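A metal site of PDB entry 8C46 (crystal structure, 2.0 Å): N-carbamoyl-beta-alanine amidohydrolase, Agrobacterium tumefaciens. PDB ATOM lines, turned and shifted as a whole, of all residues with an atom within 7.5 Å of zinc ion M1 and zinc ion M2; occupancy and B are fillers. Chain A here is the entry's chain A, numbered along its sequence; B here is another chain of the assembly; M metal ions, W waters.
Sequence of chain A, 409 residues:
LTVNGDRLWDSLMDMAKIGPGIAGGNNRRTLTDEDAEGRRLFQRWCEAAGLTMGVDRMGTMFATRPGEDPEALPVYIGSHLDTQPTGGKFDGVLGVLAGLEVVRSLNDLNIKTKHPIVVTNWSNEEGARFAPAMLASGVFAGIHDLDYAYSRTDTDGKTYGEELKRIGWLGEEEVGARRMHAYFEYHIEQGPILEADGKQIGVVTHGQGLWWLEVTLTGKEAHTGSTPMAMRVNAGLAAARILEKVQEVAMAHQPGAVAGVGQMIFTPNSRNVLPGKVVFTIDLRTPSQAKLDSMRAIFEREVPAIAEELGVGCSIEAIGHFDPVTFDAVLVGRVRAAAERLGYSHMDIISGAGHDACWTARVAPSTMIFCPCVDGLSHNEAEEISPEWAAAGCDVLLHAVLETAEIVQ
Zinc ion M1 is bound by water W1, the side-chain carboxylate of Asp 91, a ring nitrogen (NE2) of His 80, a ring nitrogen (NE2) of His 187 and water W2.
Zinc ion M1 has five donor atoms within binding distance.
Merely in contact with zinc ion M1: Glu 125 (3.5 Å) and Gly 92 (3.8 Å).
Of the 26 residues printed, 5 come within 4 Å of zinc ion M1.
Along chain A the residues within 4 Å of zinc ion M1 span positions 80 to 187.
The nearest printed residue that does not touch zinc ion M1 is Glu 126 (4.1 Å).
Water W2 lies within hydrogen-bond range of ND1 of His 355 and OE2 of Glu 125.
Water W1 lies within hydrogen-bond range of the side-chain carboxylate of Glu 125 (3.1 Å) and the side-chain amide nitrogen of Gln 190 (3.3 Å).
OE1 of Glu 125 touches zinc ion M2 (3.97 Å).
Gln 190 touches zinc ion M2.
Of the 26 residues printed, 5 come within 4 Å of zinc ion M2.
Along chain A the residues within 4 Å of zinc ion M2 span positions 91 to 379.
The nearest printed residue that does not touch zinc ion M2 is His 80 (4.3 Å).
The side-chain amide nitrogen of Gln 190 sits close to a ring nitrogen (NE2) of His 379, 3.4 Å away.
OE1 of Glu 126 sits close to NE2 of Gln 84, 3.2 Å away.
The backbone carbonyl oxygen (O) of His 80 lies within hydrogen-bond range of the backbone NH (N) of Val 93, at 3.2 Å.
NE2 of Gln 190 is in hydrogen-bond range of OG of Ser 378, 3.4 Å away.
The backbone NH (N) of Asp 91 sits at hydrogen-bond distance from the side-chain carboxylate (OE2) of Glu 383.
The backbone NH (N) of Glu 126 lies within hydrogen-bond range of the side-chain carboxylate (OD2) of Asp 82, 3.0 Å away.
The side-chain carboxylate (OD2) of Asp 91 sits close to the side-chain amide nitrogen (NE2) of Gln 190 (3.2 Å).
NE2 of His 80 sits close to OE1 of Glu 125 (3.3 Å).
Zinc ion M2 is bound by the side-chain carboxylate (OD2) of Asp 91.
Water W1 is bound to zinc ion M2, 2.2 Å away.
Zinc ion M2 is bound by OE2 of Glu 126 (2.2 Å).
Zinc ion M2 is bound by the side-chain carboxylate (OE1) of Glu 126, 2.2 Å away.
Zinc ion M2 is bound by NE2 of His 379 (2.4 Å).
Zinc ion M2 has five donor atoms within binding distance.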
ATOM      1  N   SER A  79     -25.046  20.080   5.751  1.00  0.00           N
ATOM      2  CA  SER A  79     -25.682  18.755   5.792  1.00  0.00           C
ATOM      3  C   SER A  79     -25.682  18.234   7.237  1.00  0.00           C
ATOM      4  O   SER A  79     -25.951  19.038   8.142  1.00  0.00           O
ATOM      5  CB  SER A  79     -25.058  17.818   4.800  1.00  0.00           C
ATOM      6  OG  SER A  79     -25.961  16.797   4.425  1.00  0.00           O
ATOM      7  N   HIS A  80     -25.396  16.933   7.465  1.00  0.00           N
ATOM      8  CA  HIS A  80     -25.481  16.297   8.773  1.00  0.00           C
ATOM      9  C   HIS A  80     -24.383  15.255   8.918  1.00  0.00           C
ATOM     10  O   HIS A  80     -24.080  14.540   7.971  1.00  0.00           O
ATOM     11  CB  HIS A  80     -26.848  15.631   9.003  1.00  0.00           C
ATOM     12  CG  HIS A  80     -27.184  14.583   8.023  1.00  0.00           C
ATOM     13  ND1 HIS A  80     -26.858  13.254   8.216  1.00  0.00           N
ATOM     14  CD2 HIS A  80     -27.723  14.642   6.789  1.00  0.00           C
ATOM     15  CE1 HIS A  80     -27.225  12.530   7.191  1.00  0.00           C
ATOM     16  NE2 HIS A  80     -27.751  13.331   6.326  1.00  0.00           N
ATOM     17  N   ASP A  82     -24.756  12.953  11.541  1.00  0.00           N
ATOM     18  CA  ASP A  82     -25.423  11.818  12.158  1.00  0.00           C
ATOM     19  C   ASP A  82     -25.811  10.807  11.065  1.00  0.00           C
ATOM     20  O   ASP A  82     -26.108  11.187   9.921  1.00  0.00           O
ATOM     21  CB  ASP A  82     -26.618  12.248  13.028  1.00  0.00           C
ATOM     22  CG  ASP A  82     -27.835  12.684  12.226  1.00  0.00           C
ATOM     23  OD1 ASP A  82     -27.777  13.829  11.632  1.00  0.00           O
ATOM     24  OD2 ASP A  82     -28.807  11.882  12.163  1.00  0.00           O
ATOM     25  N   THR A  83     -25.805   9.531  11.450  1.00  0.00           N
ATOM     26  CA  THR A  83     -26.010   8.440  10.507  1.00  0.00           C
ATOM     27  C   THR A  83     -27.157   7.555  10.997  1.00  0.00           C
ATOM     28  O   THR A  83     -27.627   7.634  12.132  1.00  0.00           O
ATOM     29  CB  THR A  83     -24.727   7.608  10.345  1.00  0.00           C
ATOM     30  OG1 THR A  83     -24.460   6.806  11.510  1.00  0.00           O
ATOM     31  CG2 THR A  83     -23.514   8.472  10.067  1.00  0.00           C
ATOM     32  N   GLN A  84     -27.631   6.736  10.062  1.00  0.00           N
ATOM     33  CA  GLN A  84     -28.439   5.575  10.355  1.00  0.00           C
ATOM     34  C   GLN A  84     -27.638   4.562  11.180  1.00  0.00           C
ATOM     35  O   GLN A  84     -26.398   4.551  11.152  1.00  0.00           O
ATOM     36  CB  GLN A  84     -28.869   4.997   9.011  1.00  0.00           C
ATOM     37  CG  GLN A  84     -29.895   5.874   8.273  1.00  0.00           C
ATOM     38  CD  GLN A  84     -31.280   5.752   8.885  1.00  0.00           C
ATOM     39  OE1 GLN A  84     -31.637   4.681   9.379  1.00  0.00           O
ATOM     40  NE2 GLN A  84     -32.034   6.848   8.895  1.00  0.00           N
ATOM     41  N   PHE A  90     -21.141   8.315   3.611  1.00  0.00           N
ATOM     42  CA  PHE A  90     -21.197   9.460   2.697  1.00  0.00           C
ATOM     43  C   PHE A  90     -22.497  10.258   2.861  1.00  0.00           C
ATOM     44  O   PHE A  90     -22.494  11.489   2.702  1.00  0.00           O
ATOM     45  CB  PHE A  90     -21.011   9.002   1.254  1.00  0.00           C
ATOM     46  CG  PHE A  90     -19.754   8.207   1.033  1.00  0.00           C
ATOM     47  CD1 PHE A  90     -18.517   8.829   1.179  1.00  0.00           C
ATOM     48  CD2 PHE A  90     -19.793   6.835   0.774  1.00  0.00           C
ATOM     49  CE1 PHE A  90     -17.346   8.110   1.020  1.00  0.00           C
ATOM     50  CE2 PHE A  90     -18.614   6.131   0.620  1.00  0.00           C
ATOM     51  CZ  PHE A  90     -17.400   6.767   0.708  1.00  0.00           C
ATOM     52  N   ASP A  91     -23.589   9.562   3.202  1.00  0.00           N
ATOM     53  CA  ASP A  91     -24.829  10.230   3.494  1.00  0.00           C
ATOM     54  C   ASP A  91     -24.610  11.280   4.574  1.00  0.00           C
ATOM     55  O   ASP A  91     -24.123  10.934   5.676  1.00  0.00           O
ATOM     56  CB  ASP A  91     -25.839   9.193   3.955  1.00  0.00           C
ATOM     57  CG  ASP A  91     -27.178   9.784   4.330  1.00  0.00           C
ATOM     58  OD1 ASP A  91     -27.354  11.051   4.321  1.00  0.00           O
ATOM     59  OD2 ASP A  91     -28.048   8.957   4.563  1.00  0.00           O
ATOM     60  N   GLY A  92     -24.949  12.533   4.241  1.00  0.00           N
ATOM     61  CA  GLY A  92     -24.787  13.620   5.199  1.00  0.00           C
ATOM     62  C   GLY A  92     -23.352  14.132   5.286  1.00  0.00           C
ATOM     63  O   GLY A  92     -23.074  15.321   5.107  1.00  0.00           O
ATOM     64  N   VAL A  93     -22.420  13.219   5.574  1.00  0.00           N
ATOM     65  CA  VAL A  93     -21.036  13.548   5.841  1.00  0.00           C
ATOM     66  C   VAL A  93     -20.436  14.265   4.635  1.00  0.00           C
ATOM     67  O   VAL A  93     -19.624  15.178   4.791  1.00  0.00           O
ATOM     68  CB  VAL A  93     -20.218  12.309   6.233  1.00  0.00           C
ATOM     69  CG1 VAL A  93     -18.793  12.666   6.567  1.00  0.00           C
ATOM     70  CG2 VAL A  93     -20.829  11.526   7.357  1.00  0.00           C
ATOM     71  N   GLU A 125     -30.509  14.828  11.513  1.00  0.00           N
ATOM     72  CA  GLU A 125     -31.191  14.781  10.250  1.00  0.00           C
ATOM     73  C   GLU A 125     -31.887  13.417  10.046  1.00  0.00           C
ATOM     74  O   GLU A 125     -32.973  13.449   9.446  1.00  0.00           O
ATOM     75  CB  GLU A 125     -30.271  15.026   9.057  1.00  0.00           C
ATOM     76  CG  GLU A 125     -31.081  15.216   7.784  1.00  0.00           C
ATOM     77  CD  GLU A 125     -31.532  13.948   7.077  1.00  0.00           C
ATOM     78  OE1 GLU A 125     -30.863  12.910   7.249  1.00  0.00           O
ATOM     79  OE2 GLU A 125     -32.580  14.032   6.364  1.00  0.00           O
ATOM     80  N   GLU A 126     -31.234  12.295  10.451  1.00  0.00           N
ATOM     81  CA  GLU A 126     -31.654  10.981   9.979  1.00  0.00           C
ATOM     82  C   GLU A 126     -33.042  10.529  10.503  1.00  0.00           C
ATOM     83  O   GLU A 126     -33.811   9.864   9.782  1.00  0.00           O
ATOM     84  CB  GLU A 126     -30.572   9.931  10.254  1.00  0.00           C
ATOM     85  CG  GLU A 126     -29.391  10.038   9.322  1.00  0.00           C
ATOM     86  CD  GLU A 126     -29.592   9.614   7.876  1.00  0.00           C
ATOM     87  OE1 GLU A 126     -30.729   9.363   7.393  1.00  0.00           O
ATOM     88  OE2 GLU A 126     -28.577   9.526   7.152  1.00  0.00           O
ATOM     89  N   GLY A 127     -33.366  10.882  11.746  1.00  0.00           N
ATOM     90  CA  GLY A 127     -34.642  10.507  12.346  1.00  0.00           C
ATOM     91  C   GLY A 127     -34.729   8.998  12.620  1.00  0.00           C
ATOM     92  O   GLY A 127     -35.809   8.420  12.679  1.00  0.00           O
ATOM     93  N   GLU A 185     -26.922  22.502  -0.169  1.00  0.00           N
ATOM     94  CA  GLU A 185     -26.575  21.186   0.368  1.00  0.00           C
ATOM     95  C   GLU A 185     -26.117  20.233  -0.730  1.00  0.00           C
ATOM     96  O   GLU A 185     -26.836  20.020  -1.715  1.00  0.00           O
ATOM     97  CB  GLU A 185     -27.721  20.644   1.197  1.00  0.00           C
ATOM     98  CG  GLU A 185     -27.512  19.208   1.679  1.00  0.00           C
ATOM     99  CD  GLU A 185     -28.412  18.807   2.838  1.00  0.00           C
ATOM    100  OE1 GLU A 185     -29.240  19.636   3.290  1.00  0.00           O
ATOM    101  OE2 GLU A 185     -28.157  17.692   3.357  1.00  0.00           O
ATOM    102  N   HIS A 187     -25.186  16.374  -1.447  1.00  0.00           N
ATOM    103  CA  HIS A 187     -25.549  15.065  -0.868  1.00  0.00           C
ATOM    104  C   HIS A 187     -25.466  13.967  -1.937  1.00  0.00           C
ATOM    105  O   HIS A 187     -25.590  14.240  -3.112  1.00  0.00           O
ATOM    106  CB  HIS A 187     -26.939  15.176  -0.261  1.00  0.00           C
ATOM    107  CG  HIS A 187     -27.363  14.114   0.671  1.00  0.00           C
ATOM    108  ND1 HIS A 187     -27.554  12.769   0.388  1.00  0.00           N
ATOM    109  CD2 HIS A 187     -27.601  14.293   1.993  1.00  0.00           C
ATOM    110  CE1 HIS A 187     -27.881  12.157   1.504  1.00  0.00           C
ATOM    111  NE2 HIS A 187     -27.931  13.059   2.496  1.00  0.00           N
ATOM    112  N   ILE A 188     -25.299  12.697  -1.502  1.00  0.00           N
ATOM    113  CA  ILE A 188     -25.441  11.563  -2.421  1.00  0.00           C
ATOM    114  C   ILE A 188     -26.909  11.451  -2.880  1.00  0.00           C
ATOM    115  O   ILE A 188     -27.837  11.810  -2.154  1.00  0.00           O
ATOM    116  CB  ILE A 188     -24.899  10.261  -1.797  1.00  0.00           C
ATOM    117  CG1 ILE A 188     -25.709   9.772  -0.605  1.00  0.00           C
ATOM    118  CG2 ILE A 188     -23.428  10.440  -1.405  1.00  0.00           C
ATOM    119  CD1 ILE A 188     -25.413   8.381  -0.196  1.00  0.00           C
ATOM    120  N   GLN A 190     -28.769   8.863  -3.152  1.00  0.00           N
ATOM    121  CA  GLN A 190     -29.471   7.816  -2.412  1.00  0.00           C
ATOM    122  C   GLN A 190     -30.378   7.029  -3.355  1.00  0.00           C
ATOM    123  O   GLN A 190     -31.279   6.320  -2.922  1.00  0.00           O
ATOM    124  CB  GLN A 190     -30.267   8.355  -1.213  1.00  0.00           C
ATOM    125  CG  GLN A 190     -29.449   9.098  -0.160  1.00  0.00           C
ATOM    126  CD  GLN A 190     -30.388   9.605   0.907  1.00  0.00           C
ATOM    127  OE1 GLN A 190     -31.265  10.425   0.639  1.00  0.00           O
ATOM    128  NE2 GLN A 190     -30.178   9.185   2.148  1.00  0.00           N
ATOM    129  N   ALA A 353     -35.505  11.763  -1.555  1.00  0.00           N
ATOM    130  CA  ALA A 353     -35.654  11.887  -0.106  1.00  0.00           C
ATOM    131  C   ALA A 353     -35.837  13.341   0.350  1.00  0.00           C
ATOM    132  O   ALA A 353     -35.618  14.294  -0.379  1.00  0.00           O
ATOM    133  CB  ALA A 353     -34.466  11.302   0.621  1.00  0.00           C
ATOM    134  N   GLY A 354     -36.232  13.507   1.621  1.00  0.00           N
ATOM    135  CA  GLY A 354     -36.159  14.782   2.309  1.00  0.00           C
ATOM    136  C   GLY A 354     -34.739  14.953   2.842  1.00  0.00           C
ATOM    137  O   GLY A 354     -34.038  13.986   3.034  1.00  0.00           O
ATOM    138  N   HIS A 355     -34.314  16.212   2.921  1.00  0.00           N
ATOM    139  CA  HIS A 355     -33.056  16.686   3.484  1.00  0.00           C
ATOM    140  C   HIS A 355     -33.377  17.994   4.199  1.00  0.00           C
ATOM    141  O   HIS A 355     -34.396  18.645   3.918  1.00  0.00           O
ATOM    142  CB  HIS A 355     -32.005  16.915   2.398  1.00  0.00           C
ATOM    143  CG  HIS A 355     -31.875  15.722   1.475  1.00  0.00           C
ATOM    144  ND1 HIS A 355     -31.131  14.617   1.783  1.00  0.00           N
ATOM    145  CD2 HIS A 355     -32.495  15.471   0.226  1.00  0.00           C
ATOM    146  CE1 HIS A 355     -31.200  13.760   0.732  1.00  0.00           C
ATOM    147  NE2 HIS A 355     -32.082  14.236  -0.184  1.00  0.00           N
ATOM    148  N   ASP A 356     -32.429  18.392   5.054  1.00  0.00           N
ATOM    149  CA  ASP A 356     -32.467  19.668   5.731  1.00  0.00           C
ATOM    150  C   ASP A 356     -32.711  20.813   4.736  1.00  0.00           C
ATOM    151  O   ASP A 356     -33.384  21.760   5.065  1.00  0.00           O
ATOM    152  CB  ASP A 356     -31.161  19.894   6.524  1.00  0.00           C
ATOM    153  CG  ASP A 356     -30.923  18.863   7.609  1.00  0.00           C
ATOM    154  OD1 ASP A 356     -31.832  18.716   8.417  1.00  0.00           O
ATOM    155  OD2 ASP A 356     -29.856  18.116   7.556  1.00  0.00           O
ATOM    156  N   MET A 368     -29.895  22.048  -3.829  1.00  0.00           N
ATOM    157  CA  MET A 368     -29.049  20.895  -3.571  1.00  0.00           C
ATOM    158  C   MET A 368     -28.218  20.509  -4.782  1.00  0.00           C
ATOM    159  O   MET A 368     -28.587  20.773  -5.905  1.00  0.00           O
ATOM    160  CB  MET A 368     -29.876  19.680  -3.201  1.00  0.00           C
ATOM    161  CG  MET A 368     -30.693  19.911  -1.949  1.00  0.00           C
ATOM    162  SD  MET A 368     -31.366  18.379  -1.352  1.00  0.00           S
ATOM    163  CE  MET A 368     -29.992  17.814  -0.365  1.00  0.00           C
ATOM    164  N   SER A 378     -28.156   3.417  -0.222  1.00  0.00           N
ATOM    165  CA  SER A 378     -27.955   4.327   0.907  1.00  0.00           C
ATOM    166  C   SER A 378     -28.659   3.737   2.122  1.00  0.00           C
ATOM    167  O   SER A 378     -29.287   2.707   1.999  1.00  0.00           O
ATOM    168  CB  SER A 378     -28.433   5.763   0.612  1.00  0.00           C
ATOM    169  OG  SER A 378     -28.032   6.653   1.659  1.00  0.00           O
ATOM    170  N   HIS A 379     -28.406   4.320   3.305  1.00  0.00           N
ATOM    171  CA  HIS A 379     -28.940   3.841   4.591  1.00  0.00           C
ATOM    172  C   HIS A 379     -28.496   2.396   4.850  1.00  0.00           C
ATOM    173  O   HIS A 379     -29.252   1.619   5.434  1.00  0.00           O
ATOM    174  CB  HIS A 379     -30.470   3.978   4.689  1.00  0.00           C
ATOM    175  CG  HIS A 379     -30.930   5.374   4.840  1.00  0.00           C
ATOM    176  ND1 HIS A 379     -32.103   5.686   5.455  1.00  0.00           N
ATOM    177  CD2 HIS A 379     -30.290   6.566   4.605  1.00  0.00           C
ATOM    178  CE1 HIS A 379     -32.220   7.019   5.497  1.00  0.00           C
ATOM    179  NE2 HIS A 379     -31.114   7.552   5.006  1.00  0.00           N
ATOM    180  N   GLU A 383     -23.004   1.566   1.223  1.00  0.00           N
ATOM    181  CA  GLU A 383     -23.208   2.805   0.481  1.00  0.00           C
ATOM    182  C   GLU A 383     -21.859   3.320  -0.011  1.00  0.00           C
ATOM    183  O   GLU A 383     -20.896   3.404   0.778  1.00  0.00           O
ATOM    184  CB  GLU A 383     -23.917   3.807   1.402  1.00  0.00           C
ATOM    185  CG  GLU A 383     -23.966   5.238   0.877  1.00  0.00           C
ATOM    186  CD  GLU A 383     -24.311   6.203   1.984  1.00  0.00           C
ATOM    187  OE1 GLU A 383     -25.521   6.313   2.318  1.00  0.00           O
ATOM    188  OE2 GLU A 383     -23.348   6.779   2.563  1.00  0.00           O
ATOM    189  N   HIS B 223     -33.965   3.102  -0.604  1.00  0.00           N
ATOM    190  CA  HIS B 223     -34.731   4.192  -0.035  1.00  0.00           C
ATOM    191  C   HIS B 223     -36.078   4.259  -0.780  1.00  0.00           C
ATOM    192  O   HIS B 223     -36.132   4.251  -1.989  1.00  0.00           O
ATOM    193  CB  HIS B 223     -33.862   5.466  -0.103  1.00  0.00           C
ATOM    194  CG  HIS B 223     -34.318   6.537   0.779  1.00  0.00           C
ATOM    195  ND1 HIS B 223     -35.491   7.231   0.548  1.00  0.00           N
ATOM    196  CD2 HIS B 223     -33.767   7.018   1.909  1.00  0.00           C
ATOM    197  CE1 HIS B 223     -35.695   8.044   1.553  1.00  0.00           C
ATOM    198  NE2 HIS B 223     -34.633   7.986   2.374  1.00  0.00           N
ATOM    199  N   ASN B 272     -38.569   4.001   5.621  1.00  0.00           N
ATOM    200  CA  ASN B 272     -38.076   4.621   4.384  1.00  0.00           C
ATOM    201  C   ASN B 272     -37.078   3.716   3.648  1.00  0.00           C
ATOM    202  O   ASN B 272     -36.298   4.195   2.824  1.00  0.00           O
ATOM    203  CB  ASN B 272     -37.551   6.002   4.650  1.00  0.00           C
ATOM    204  CG  ASN B 272     -36.430   5.982   5.670  1.00  0.00           C
ATOM    205  OD1 ASN B 272     -36.078   4.931   6.192  1.00  0.00           O
ATOM    206  ND2 ASN B 272     -35.913   7.121   6.034  1.00  0.00           N
HETATM  207 ZN    ZN M   1     -28.722  12.658   4.529  1.00  0.00          ZN
HETATM  208 ZN    ZN M   2     -29.802   9.577   5.373  1.00  0.00          ZN
HETATM  209  O   HOH W   1     -30.319  11.494   4.522  1.00  0.00           O
HETATM  210  O   HOH W   2     -30.037  14.506   4.299  1.00  0.00           O
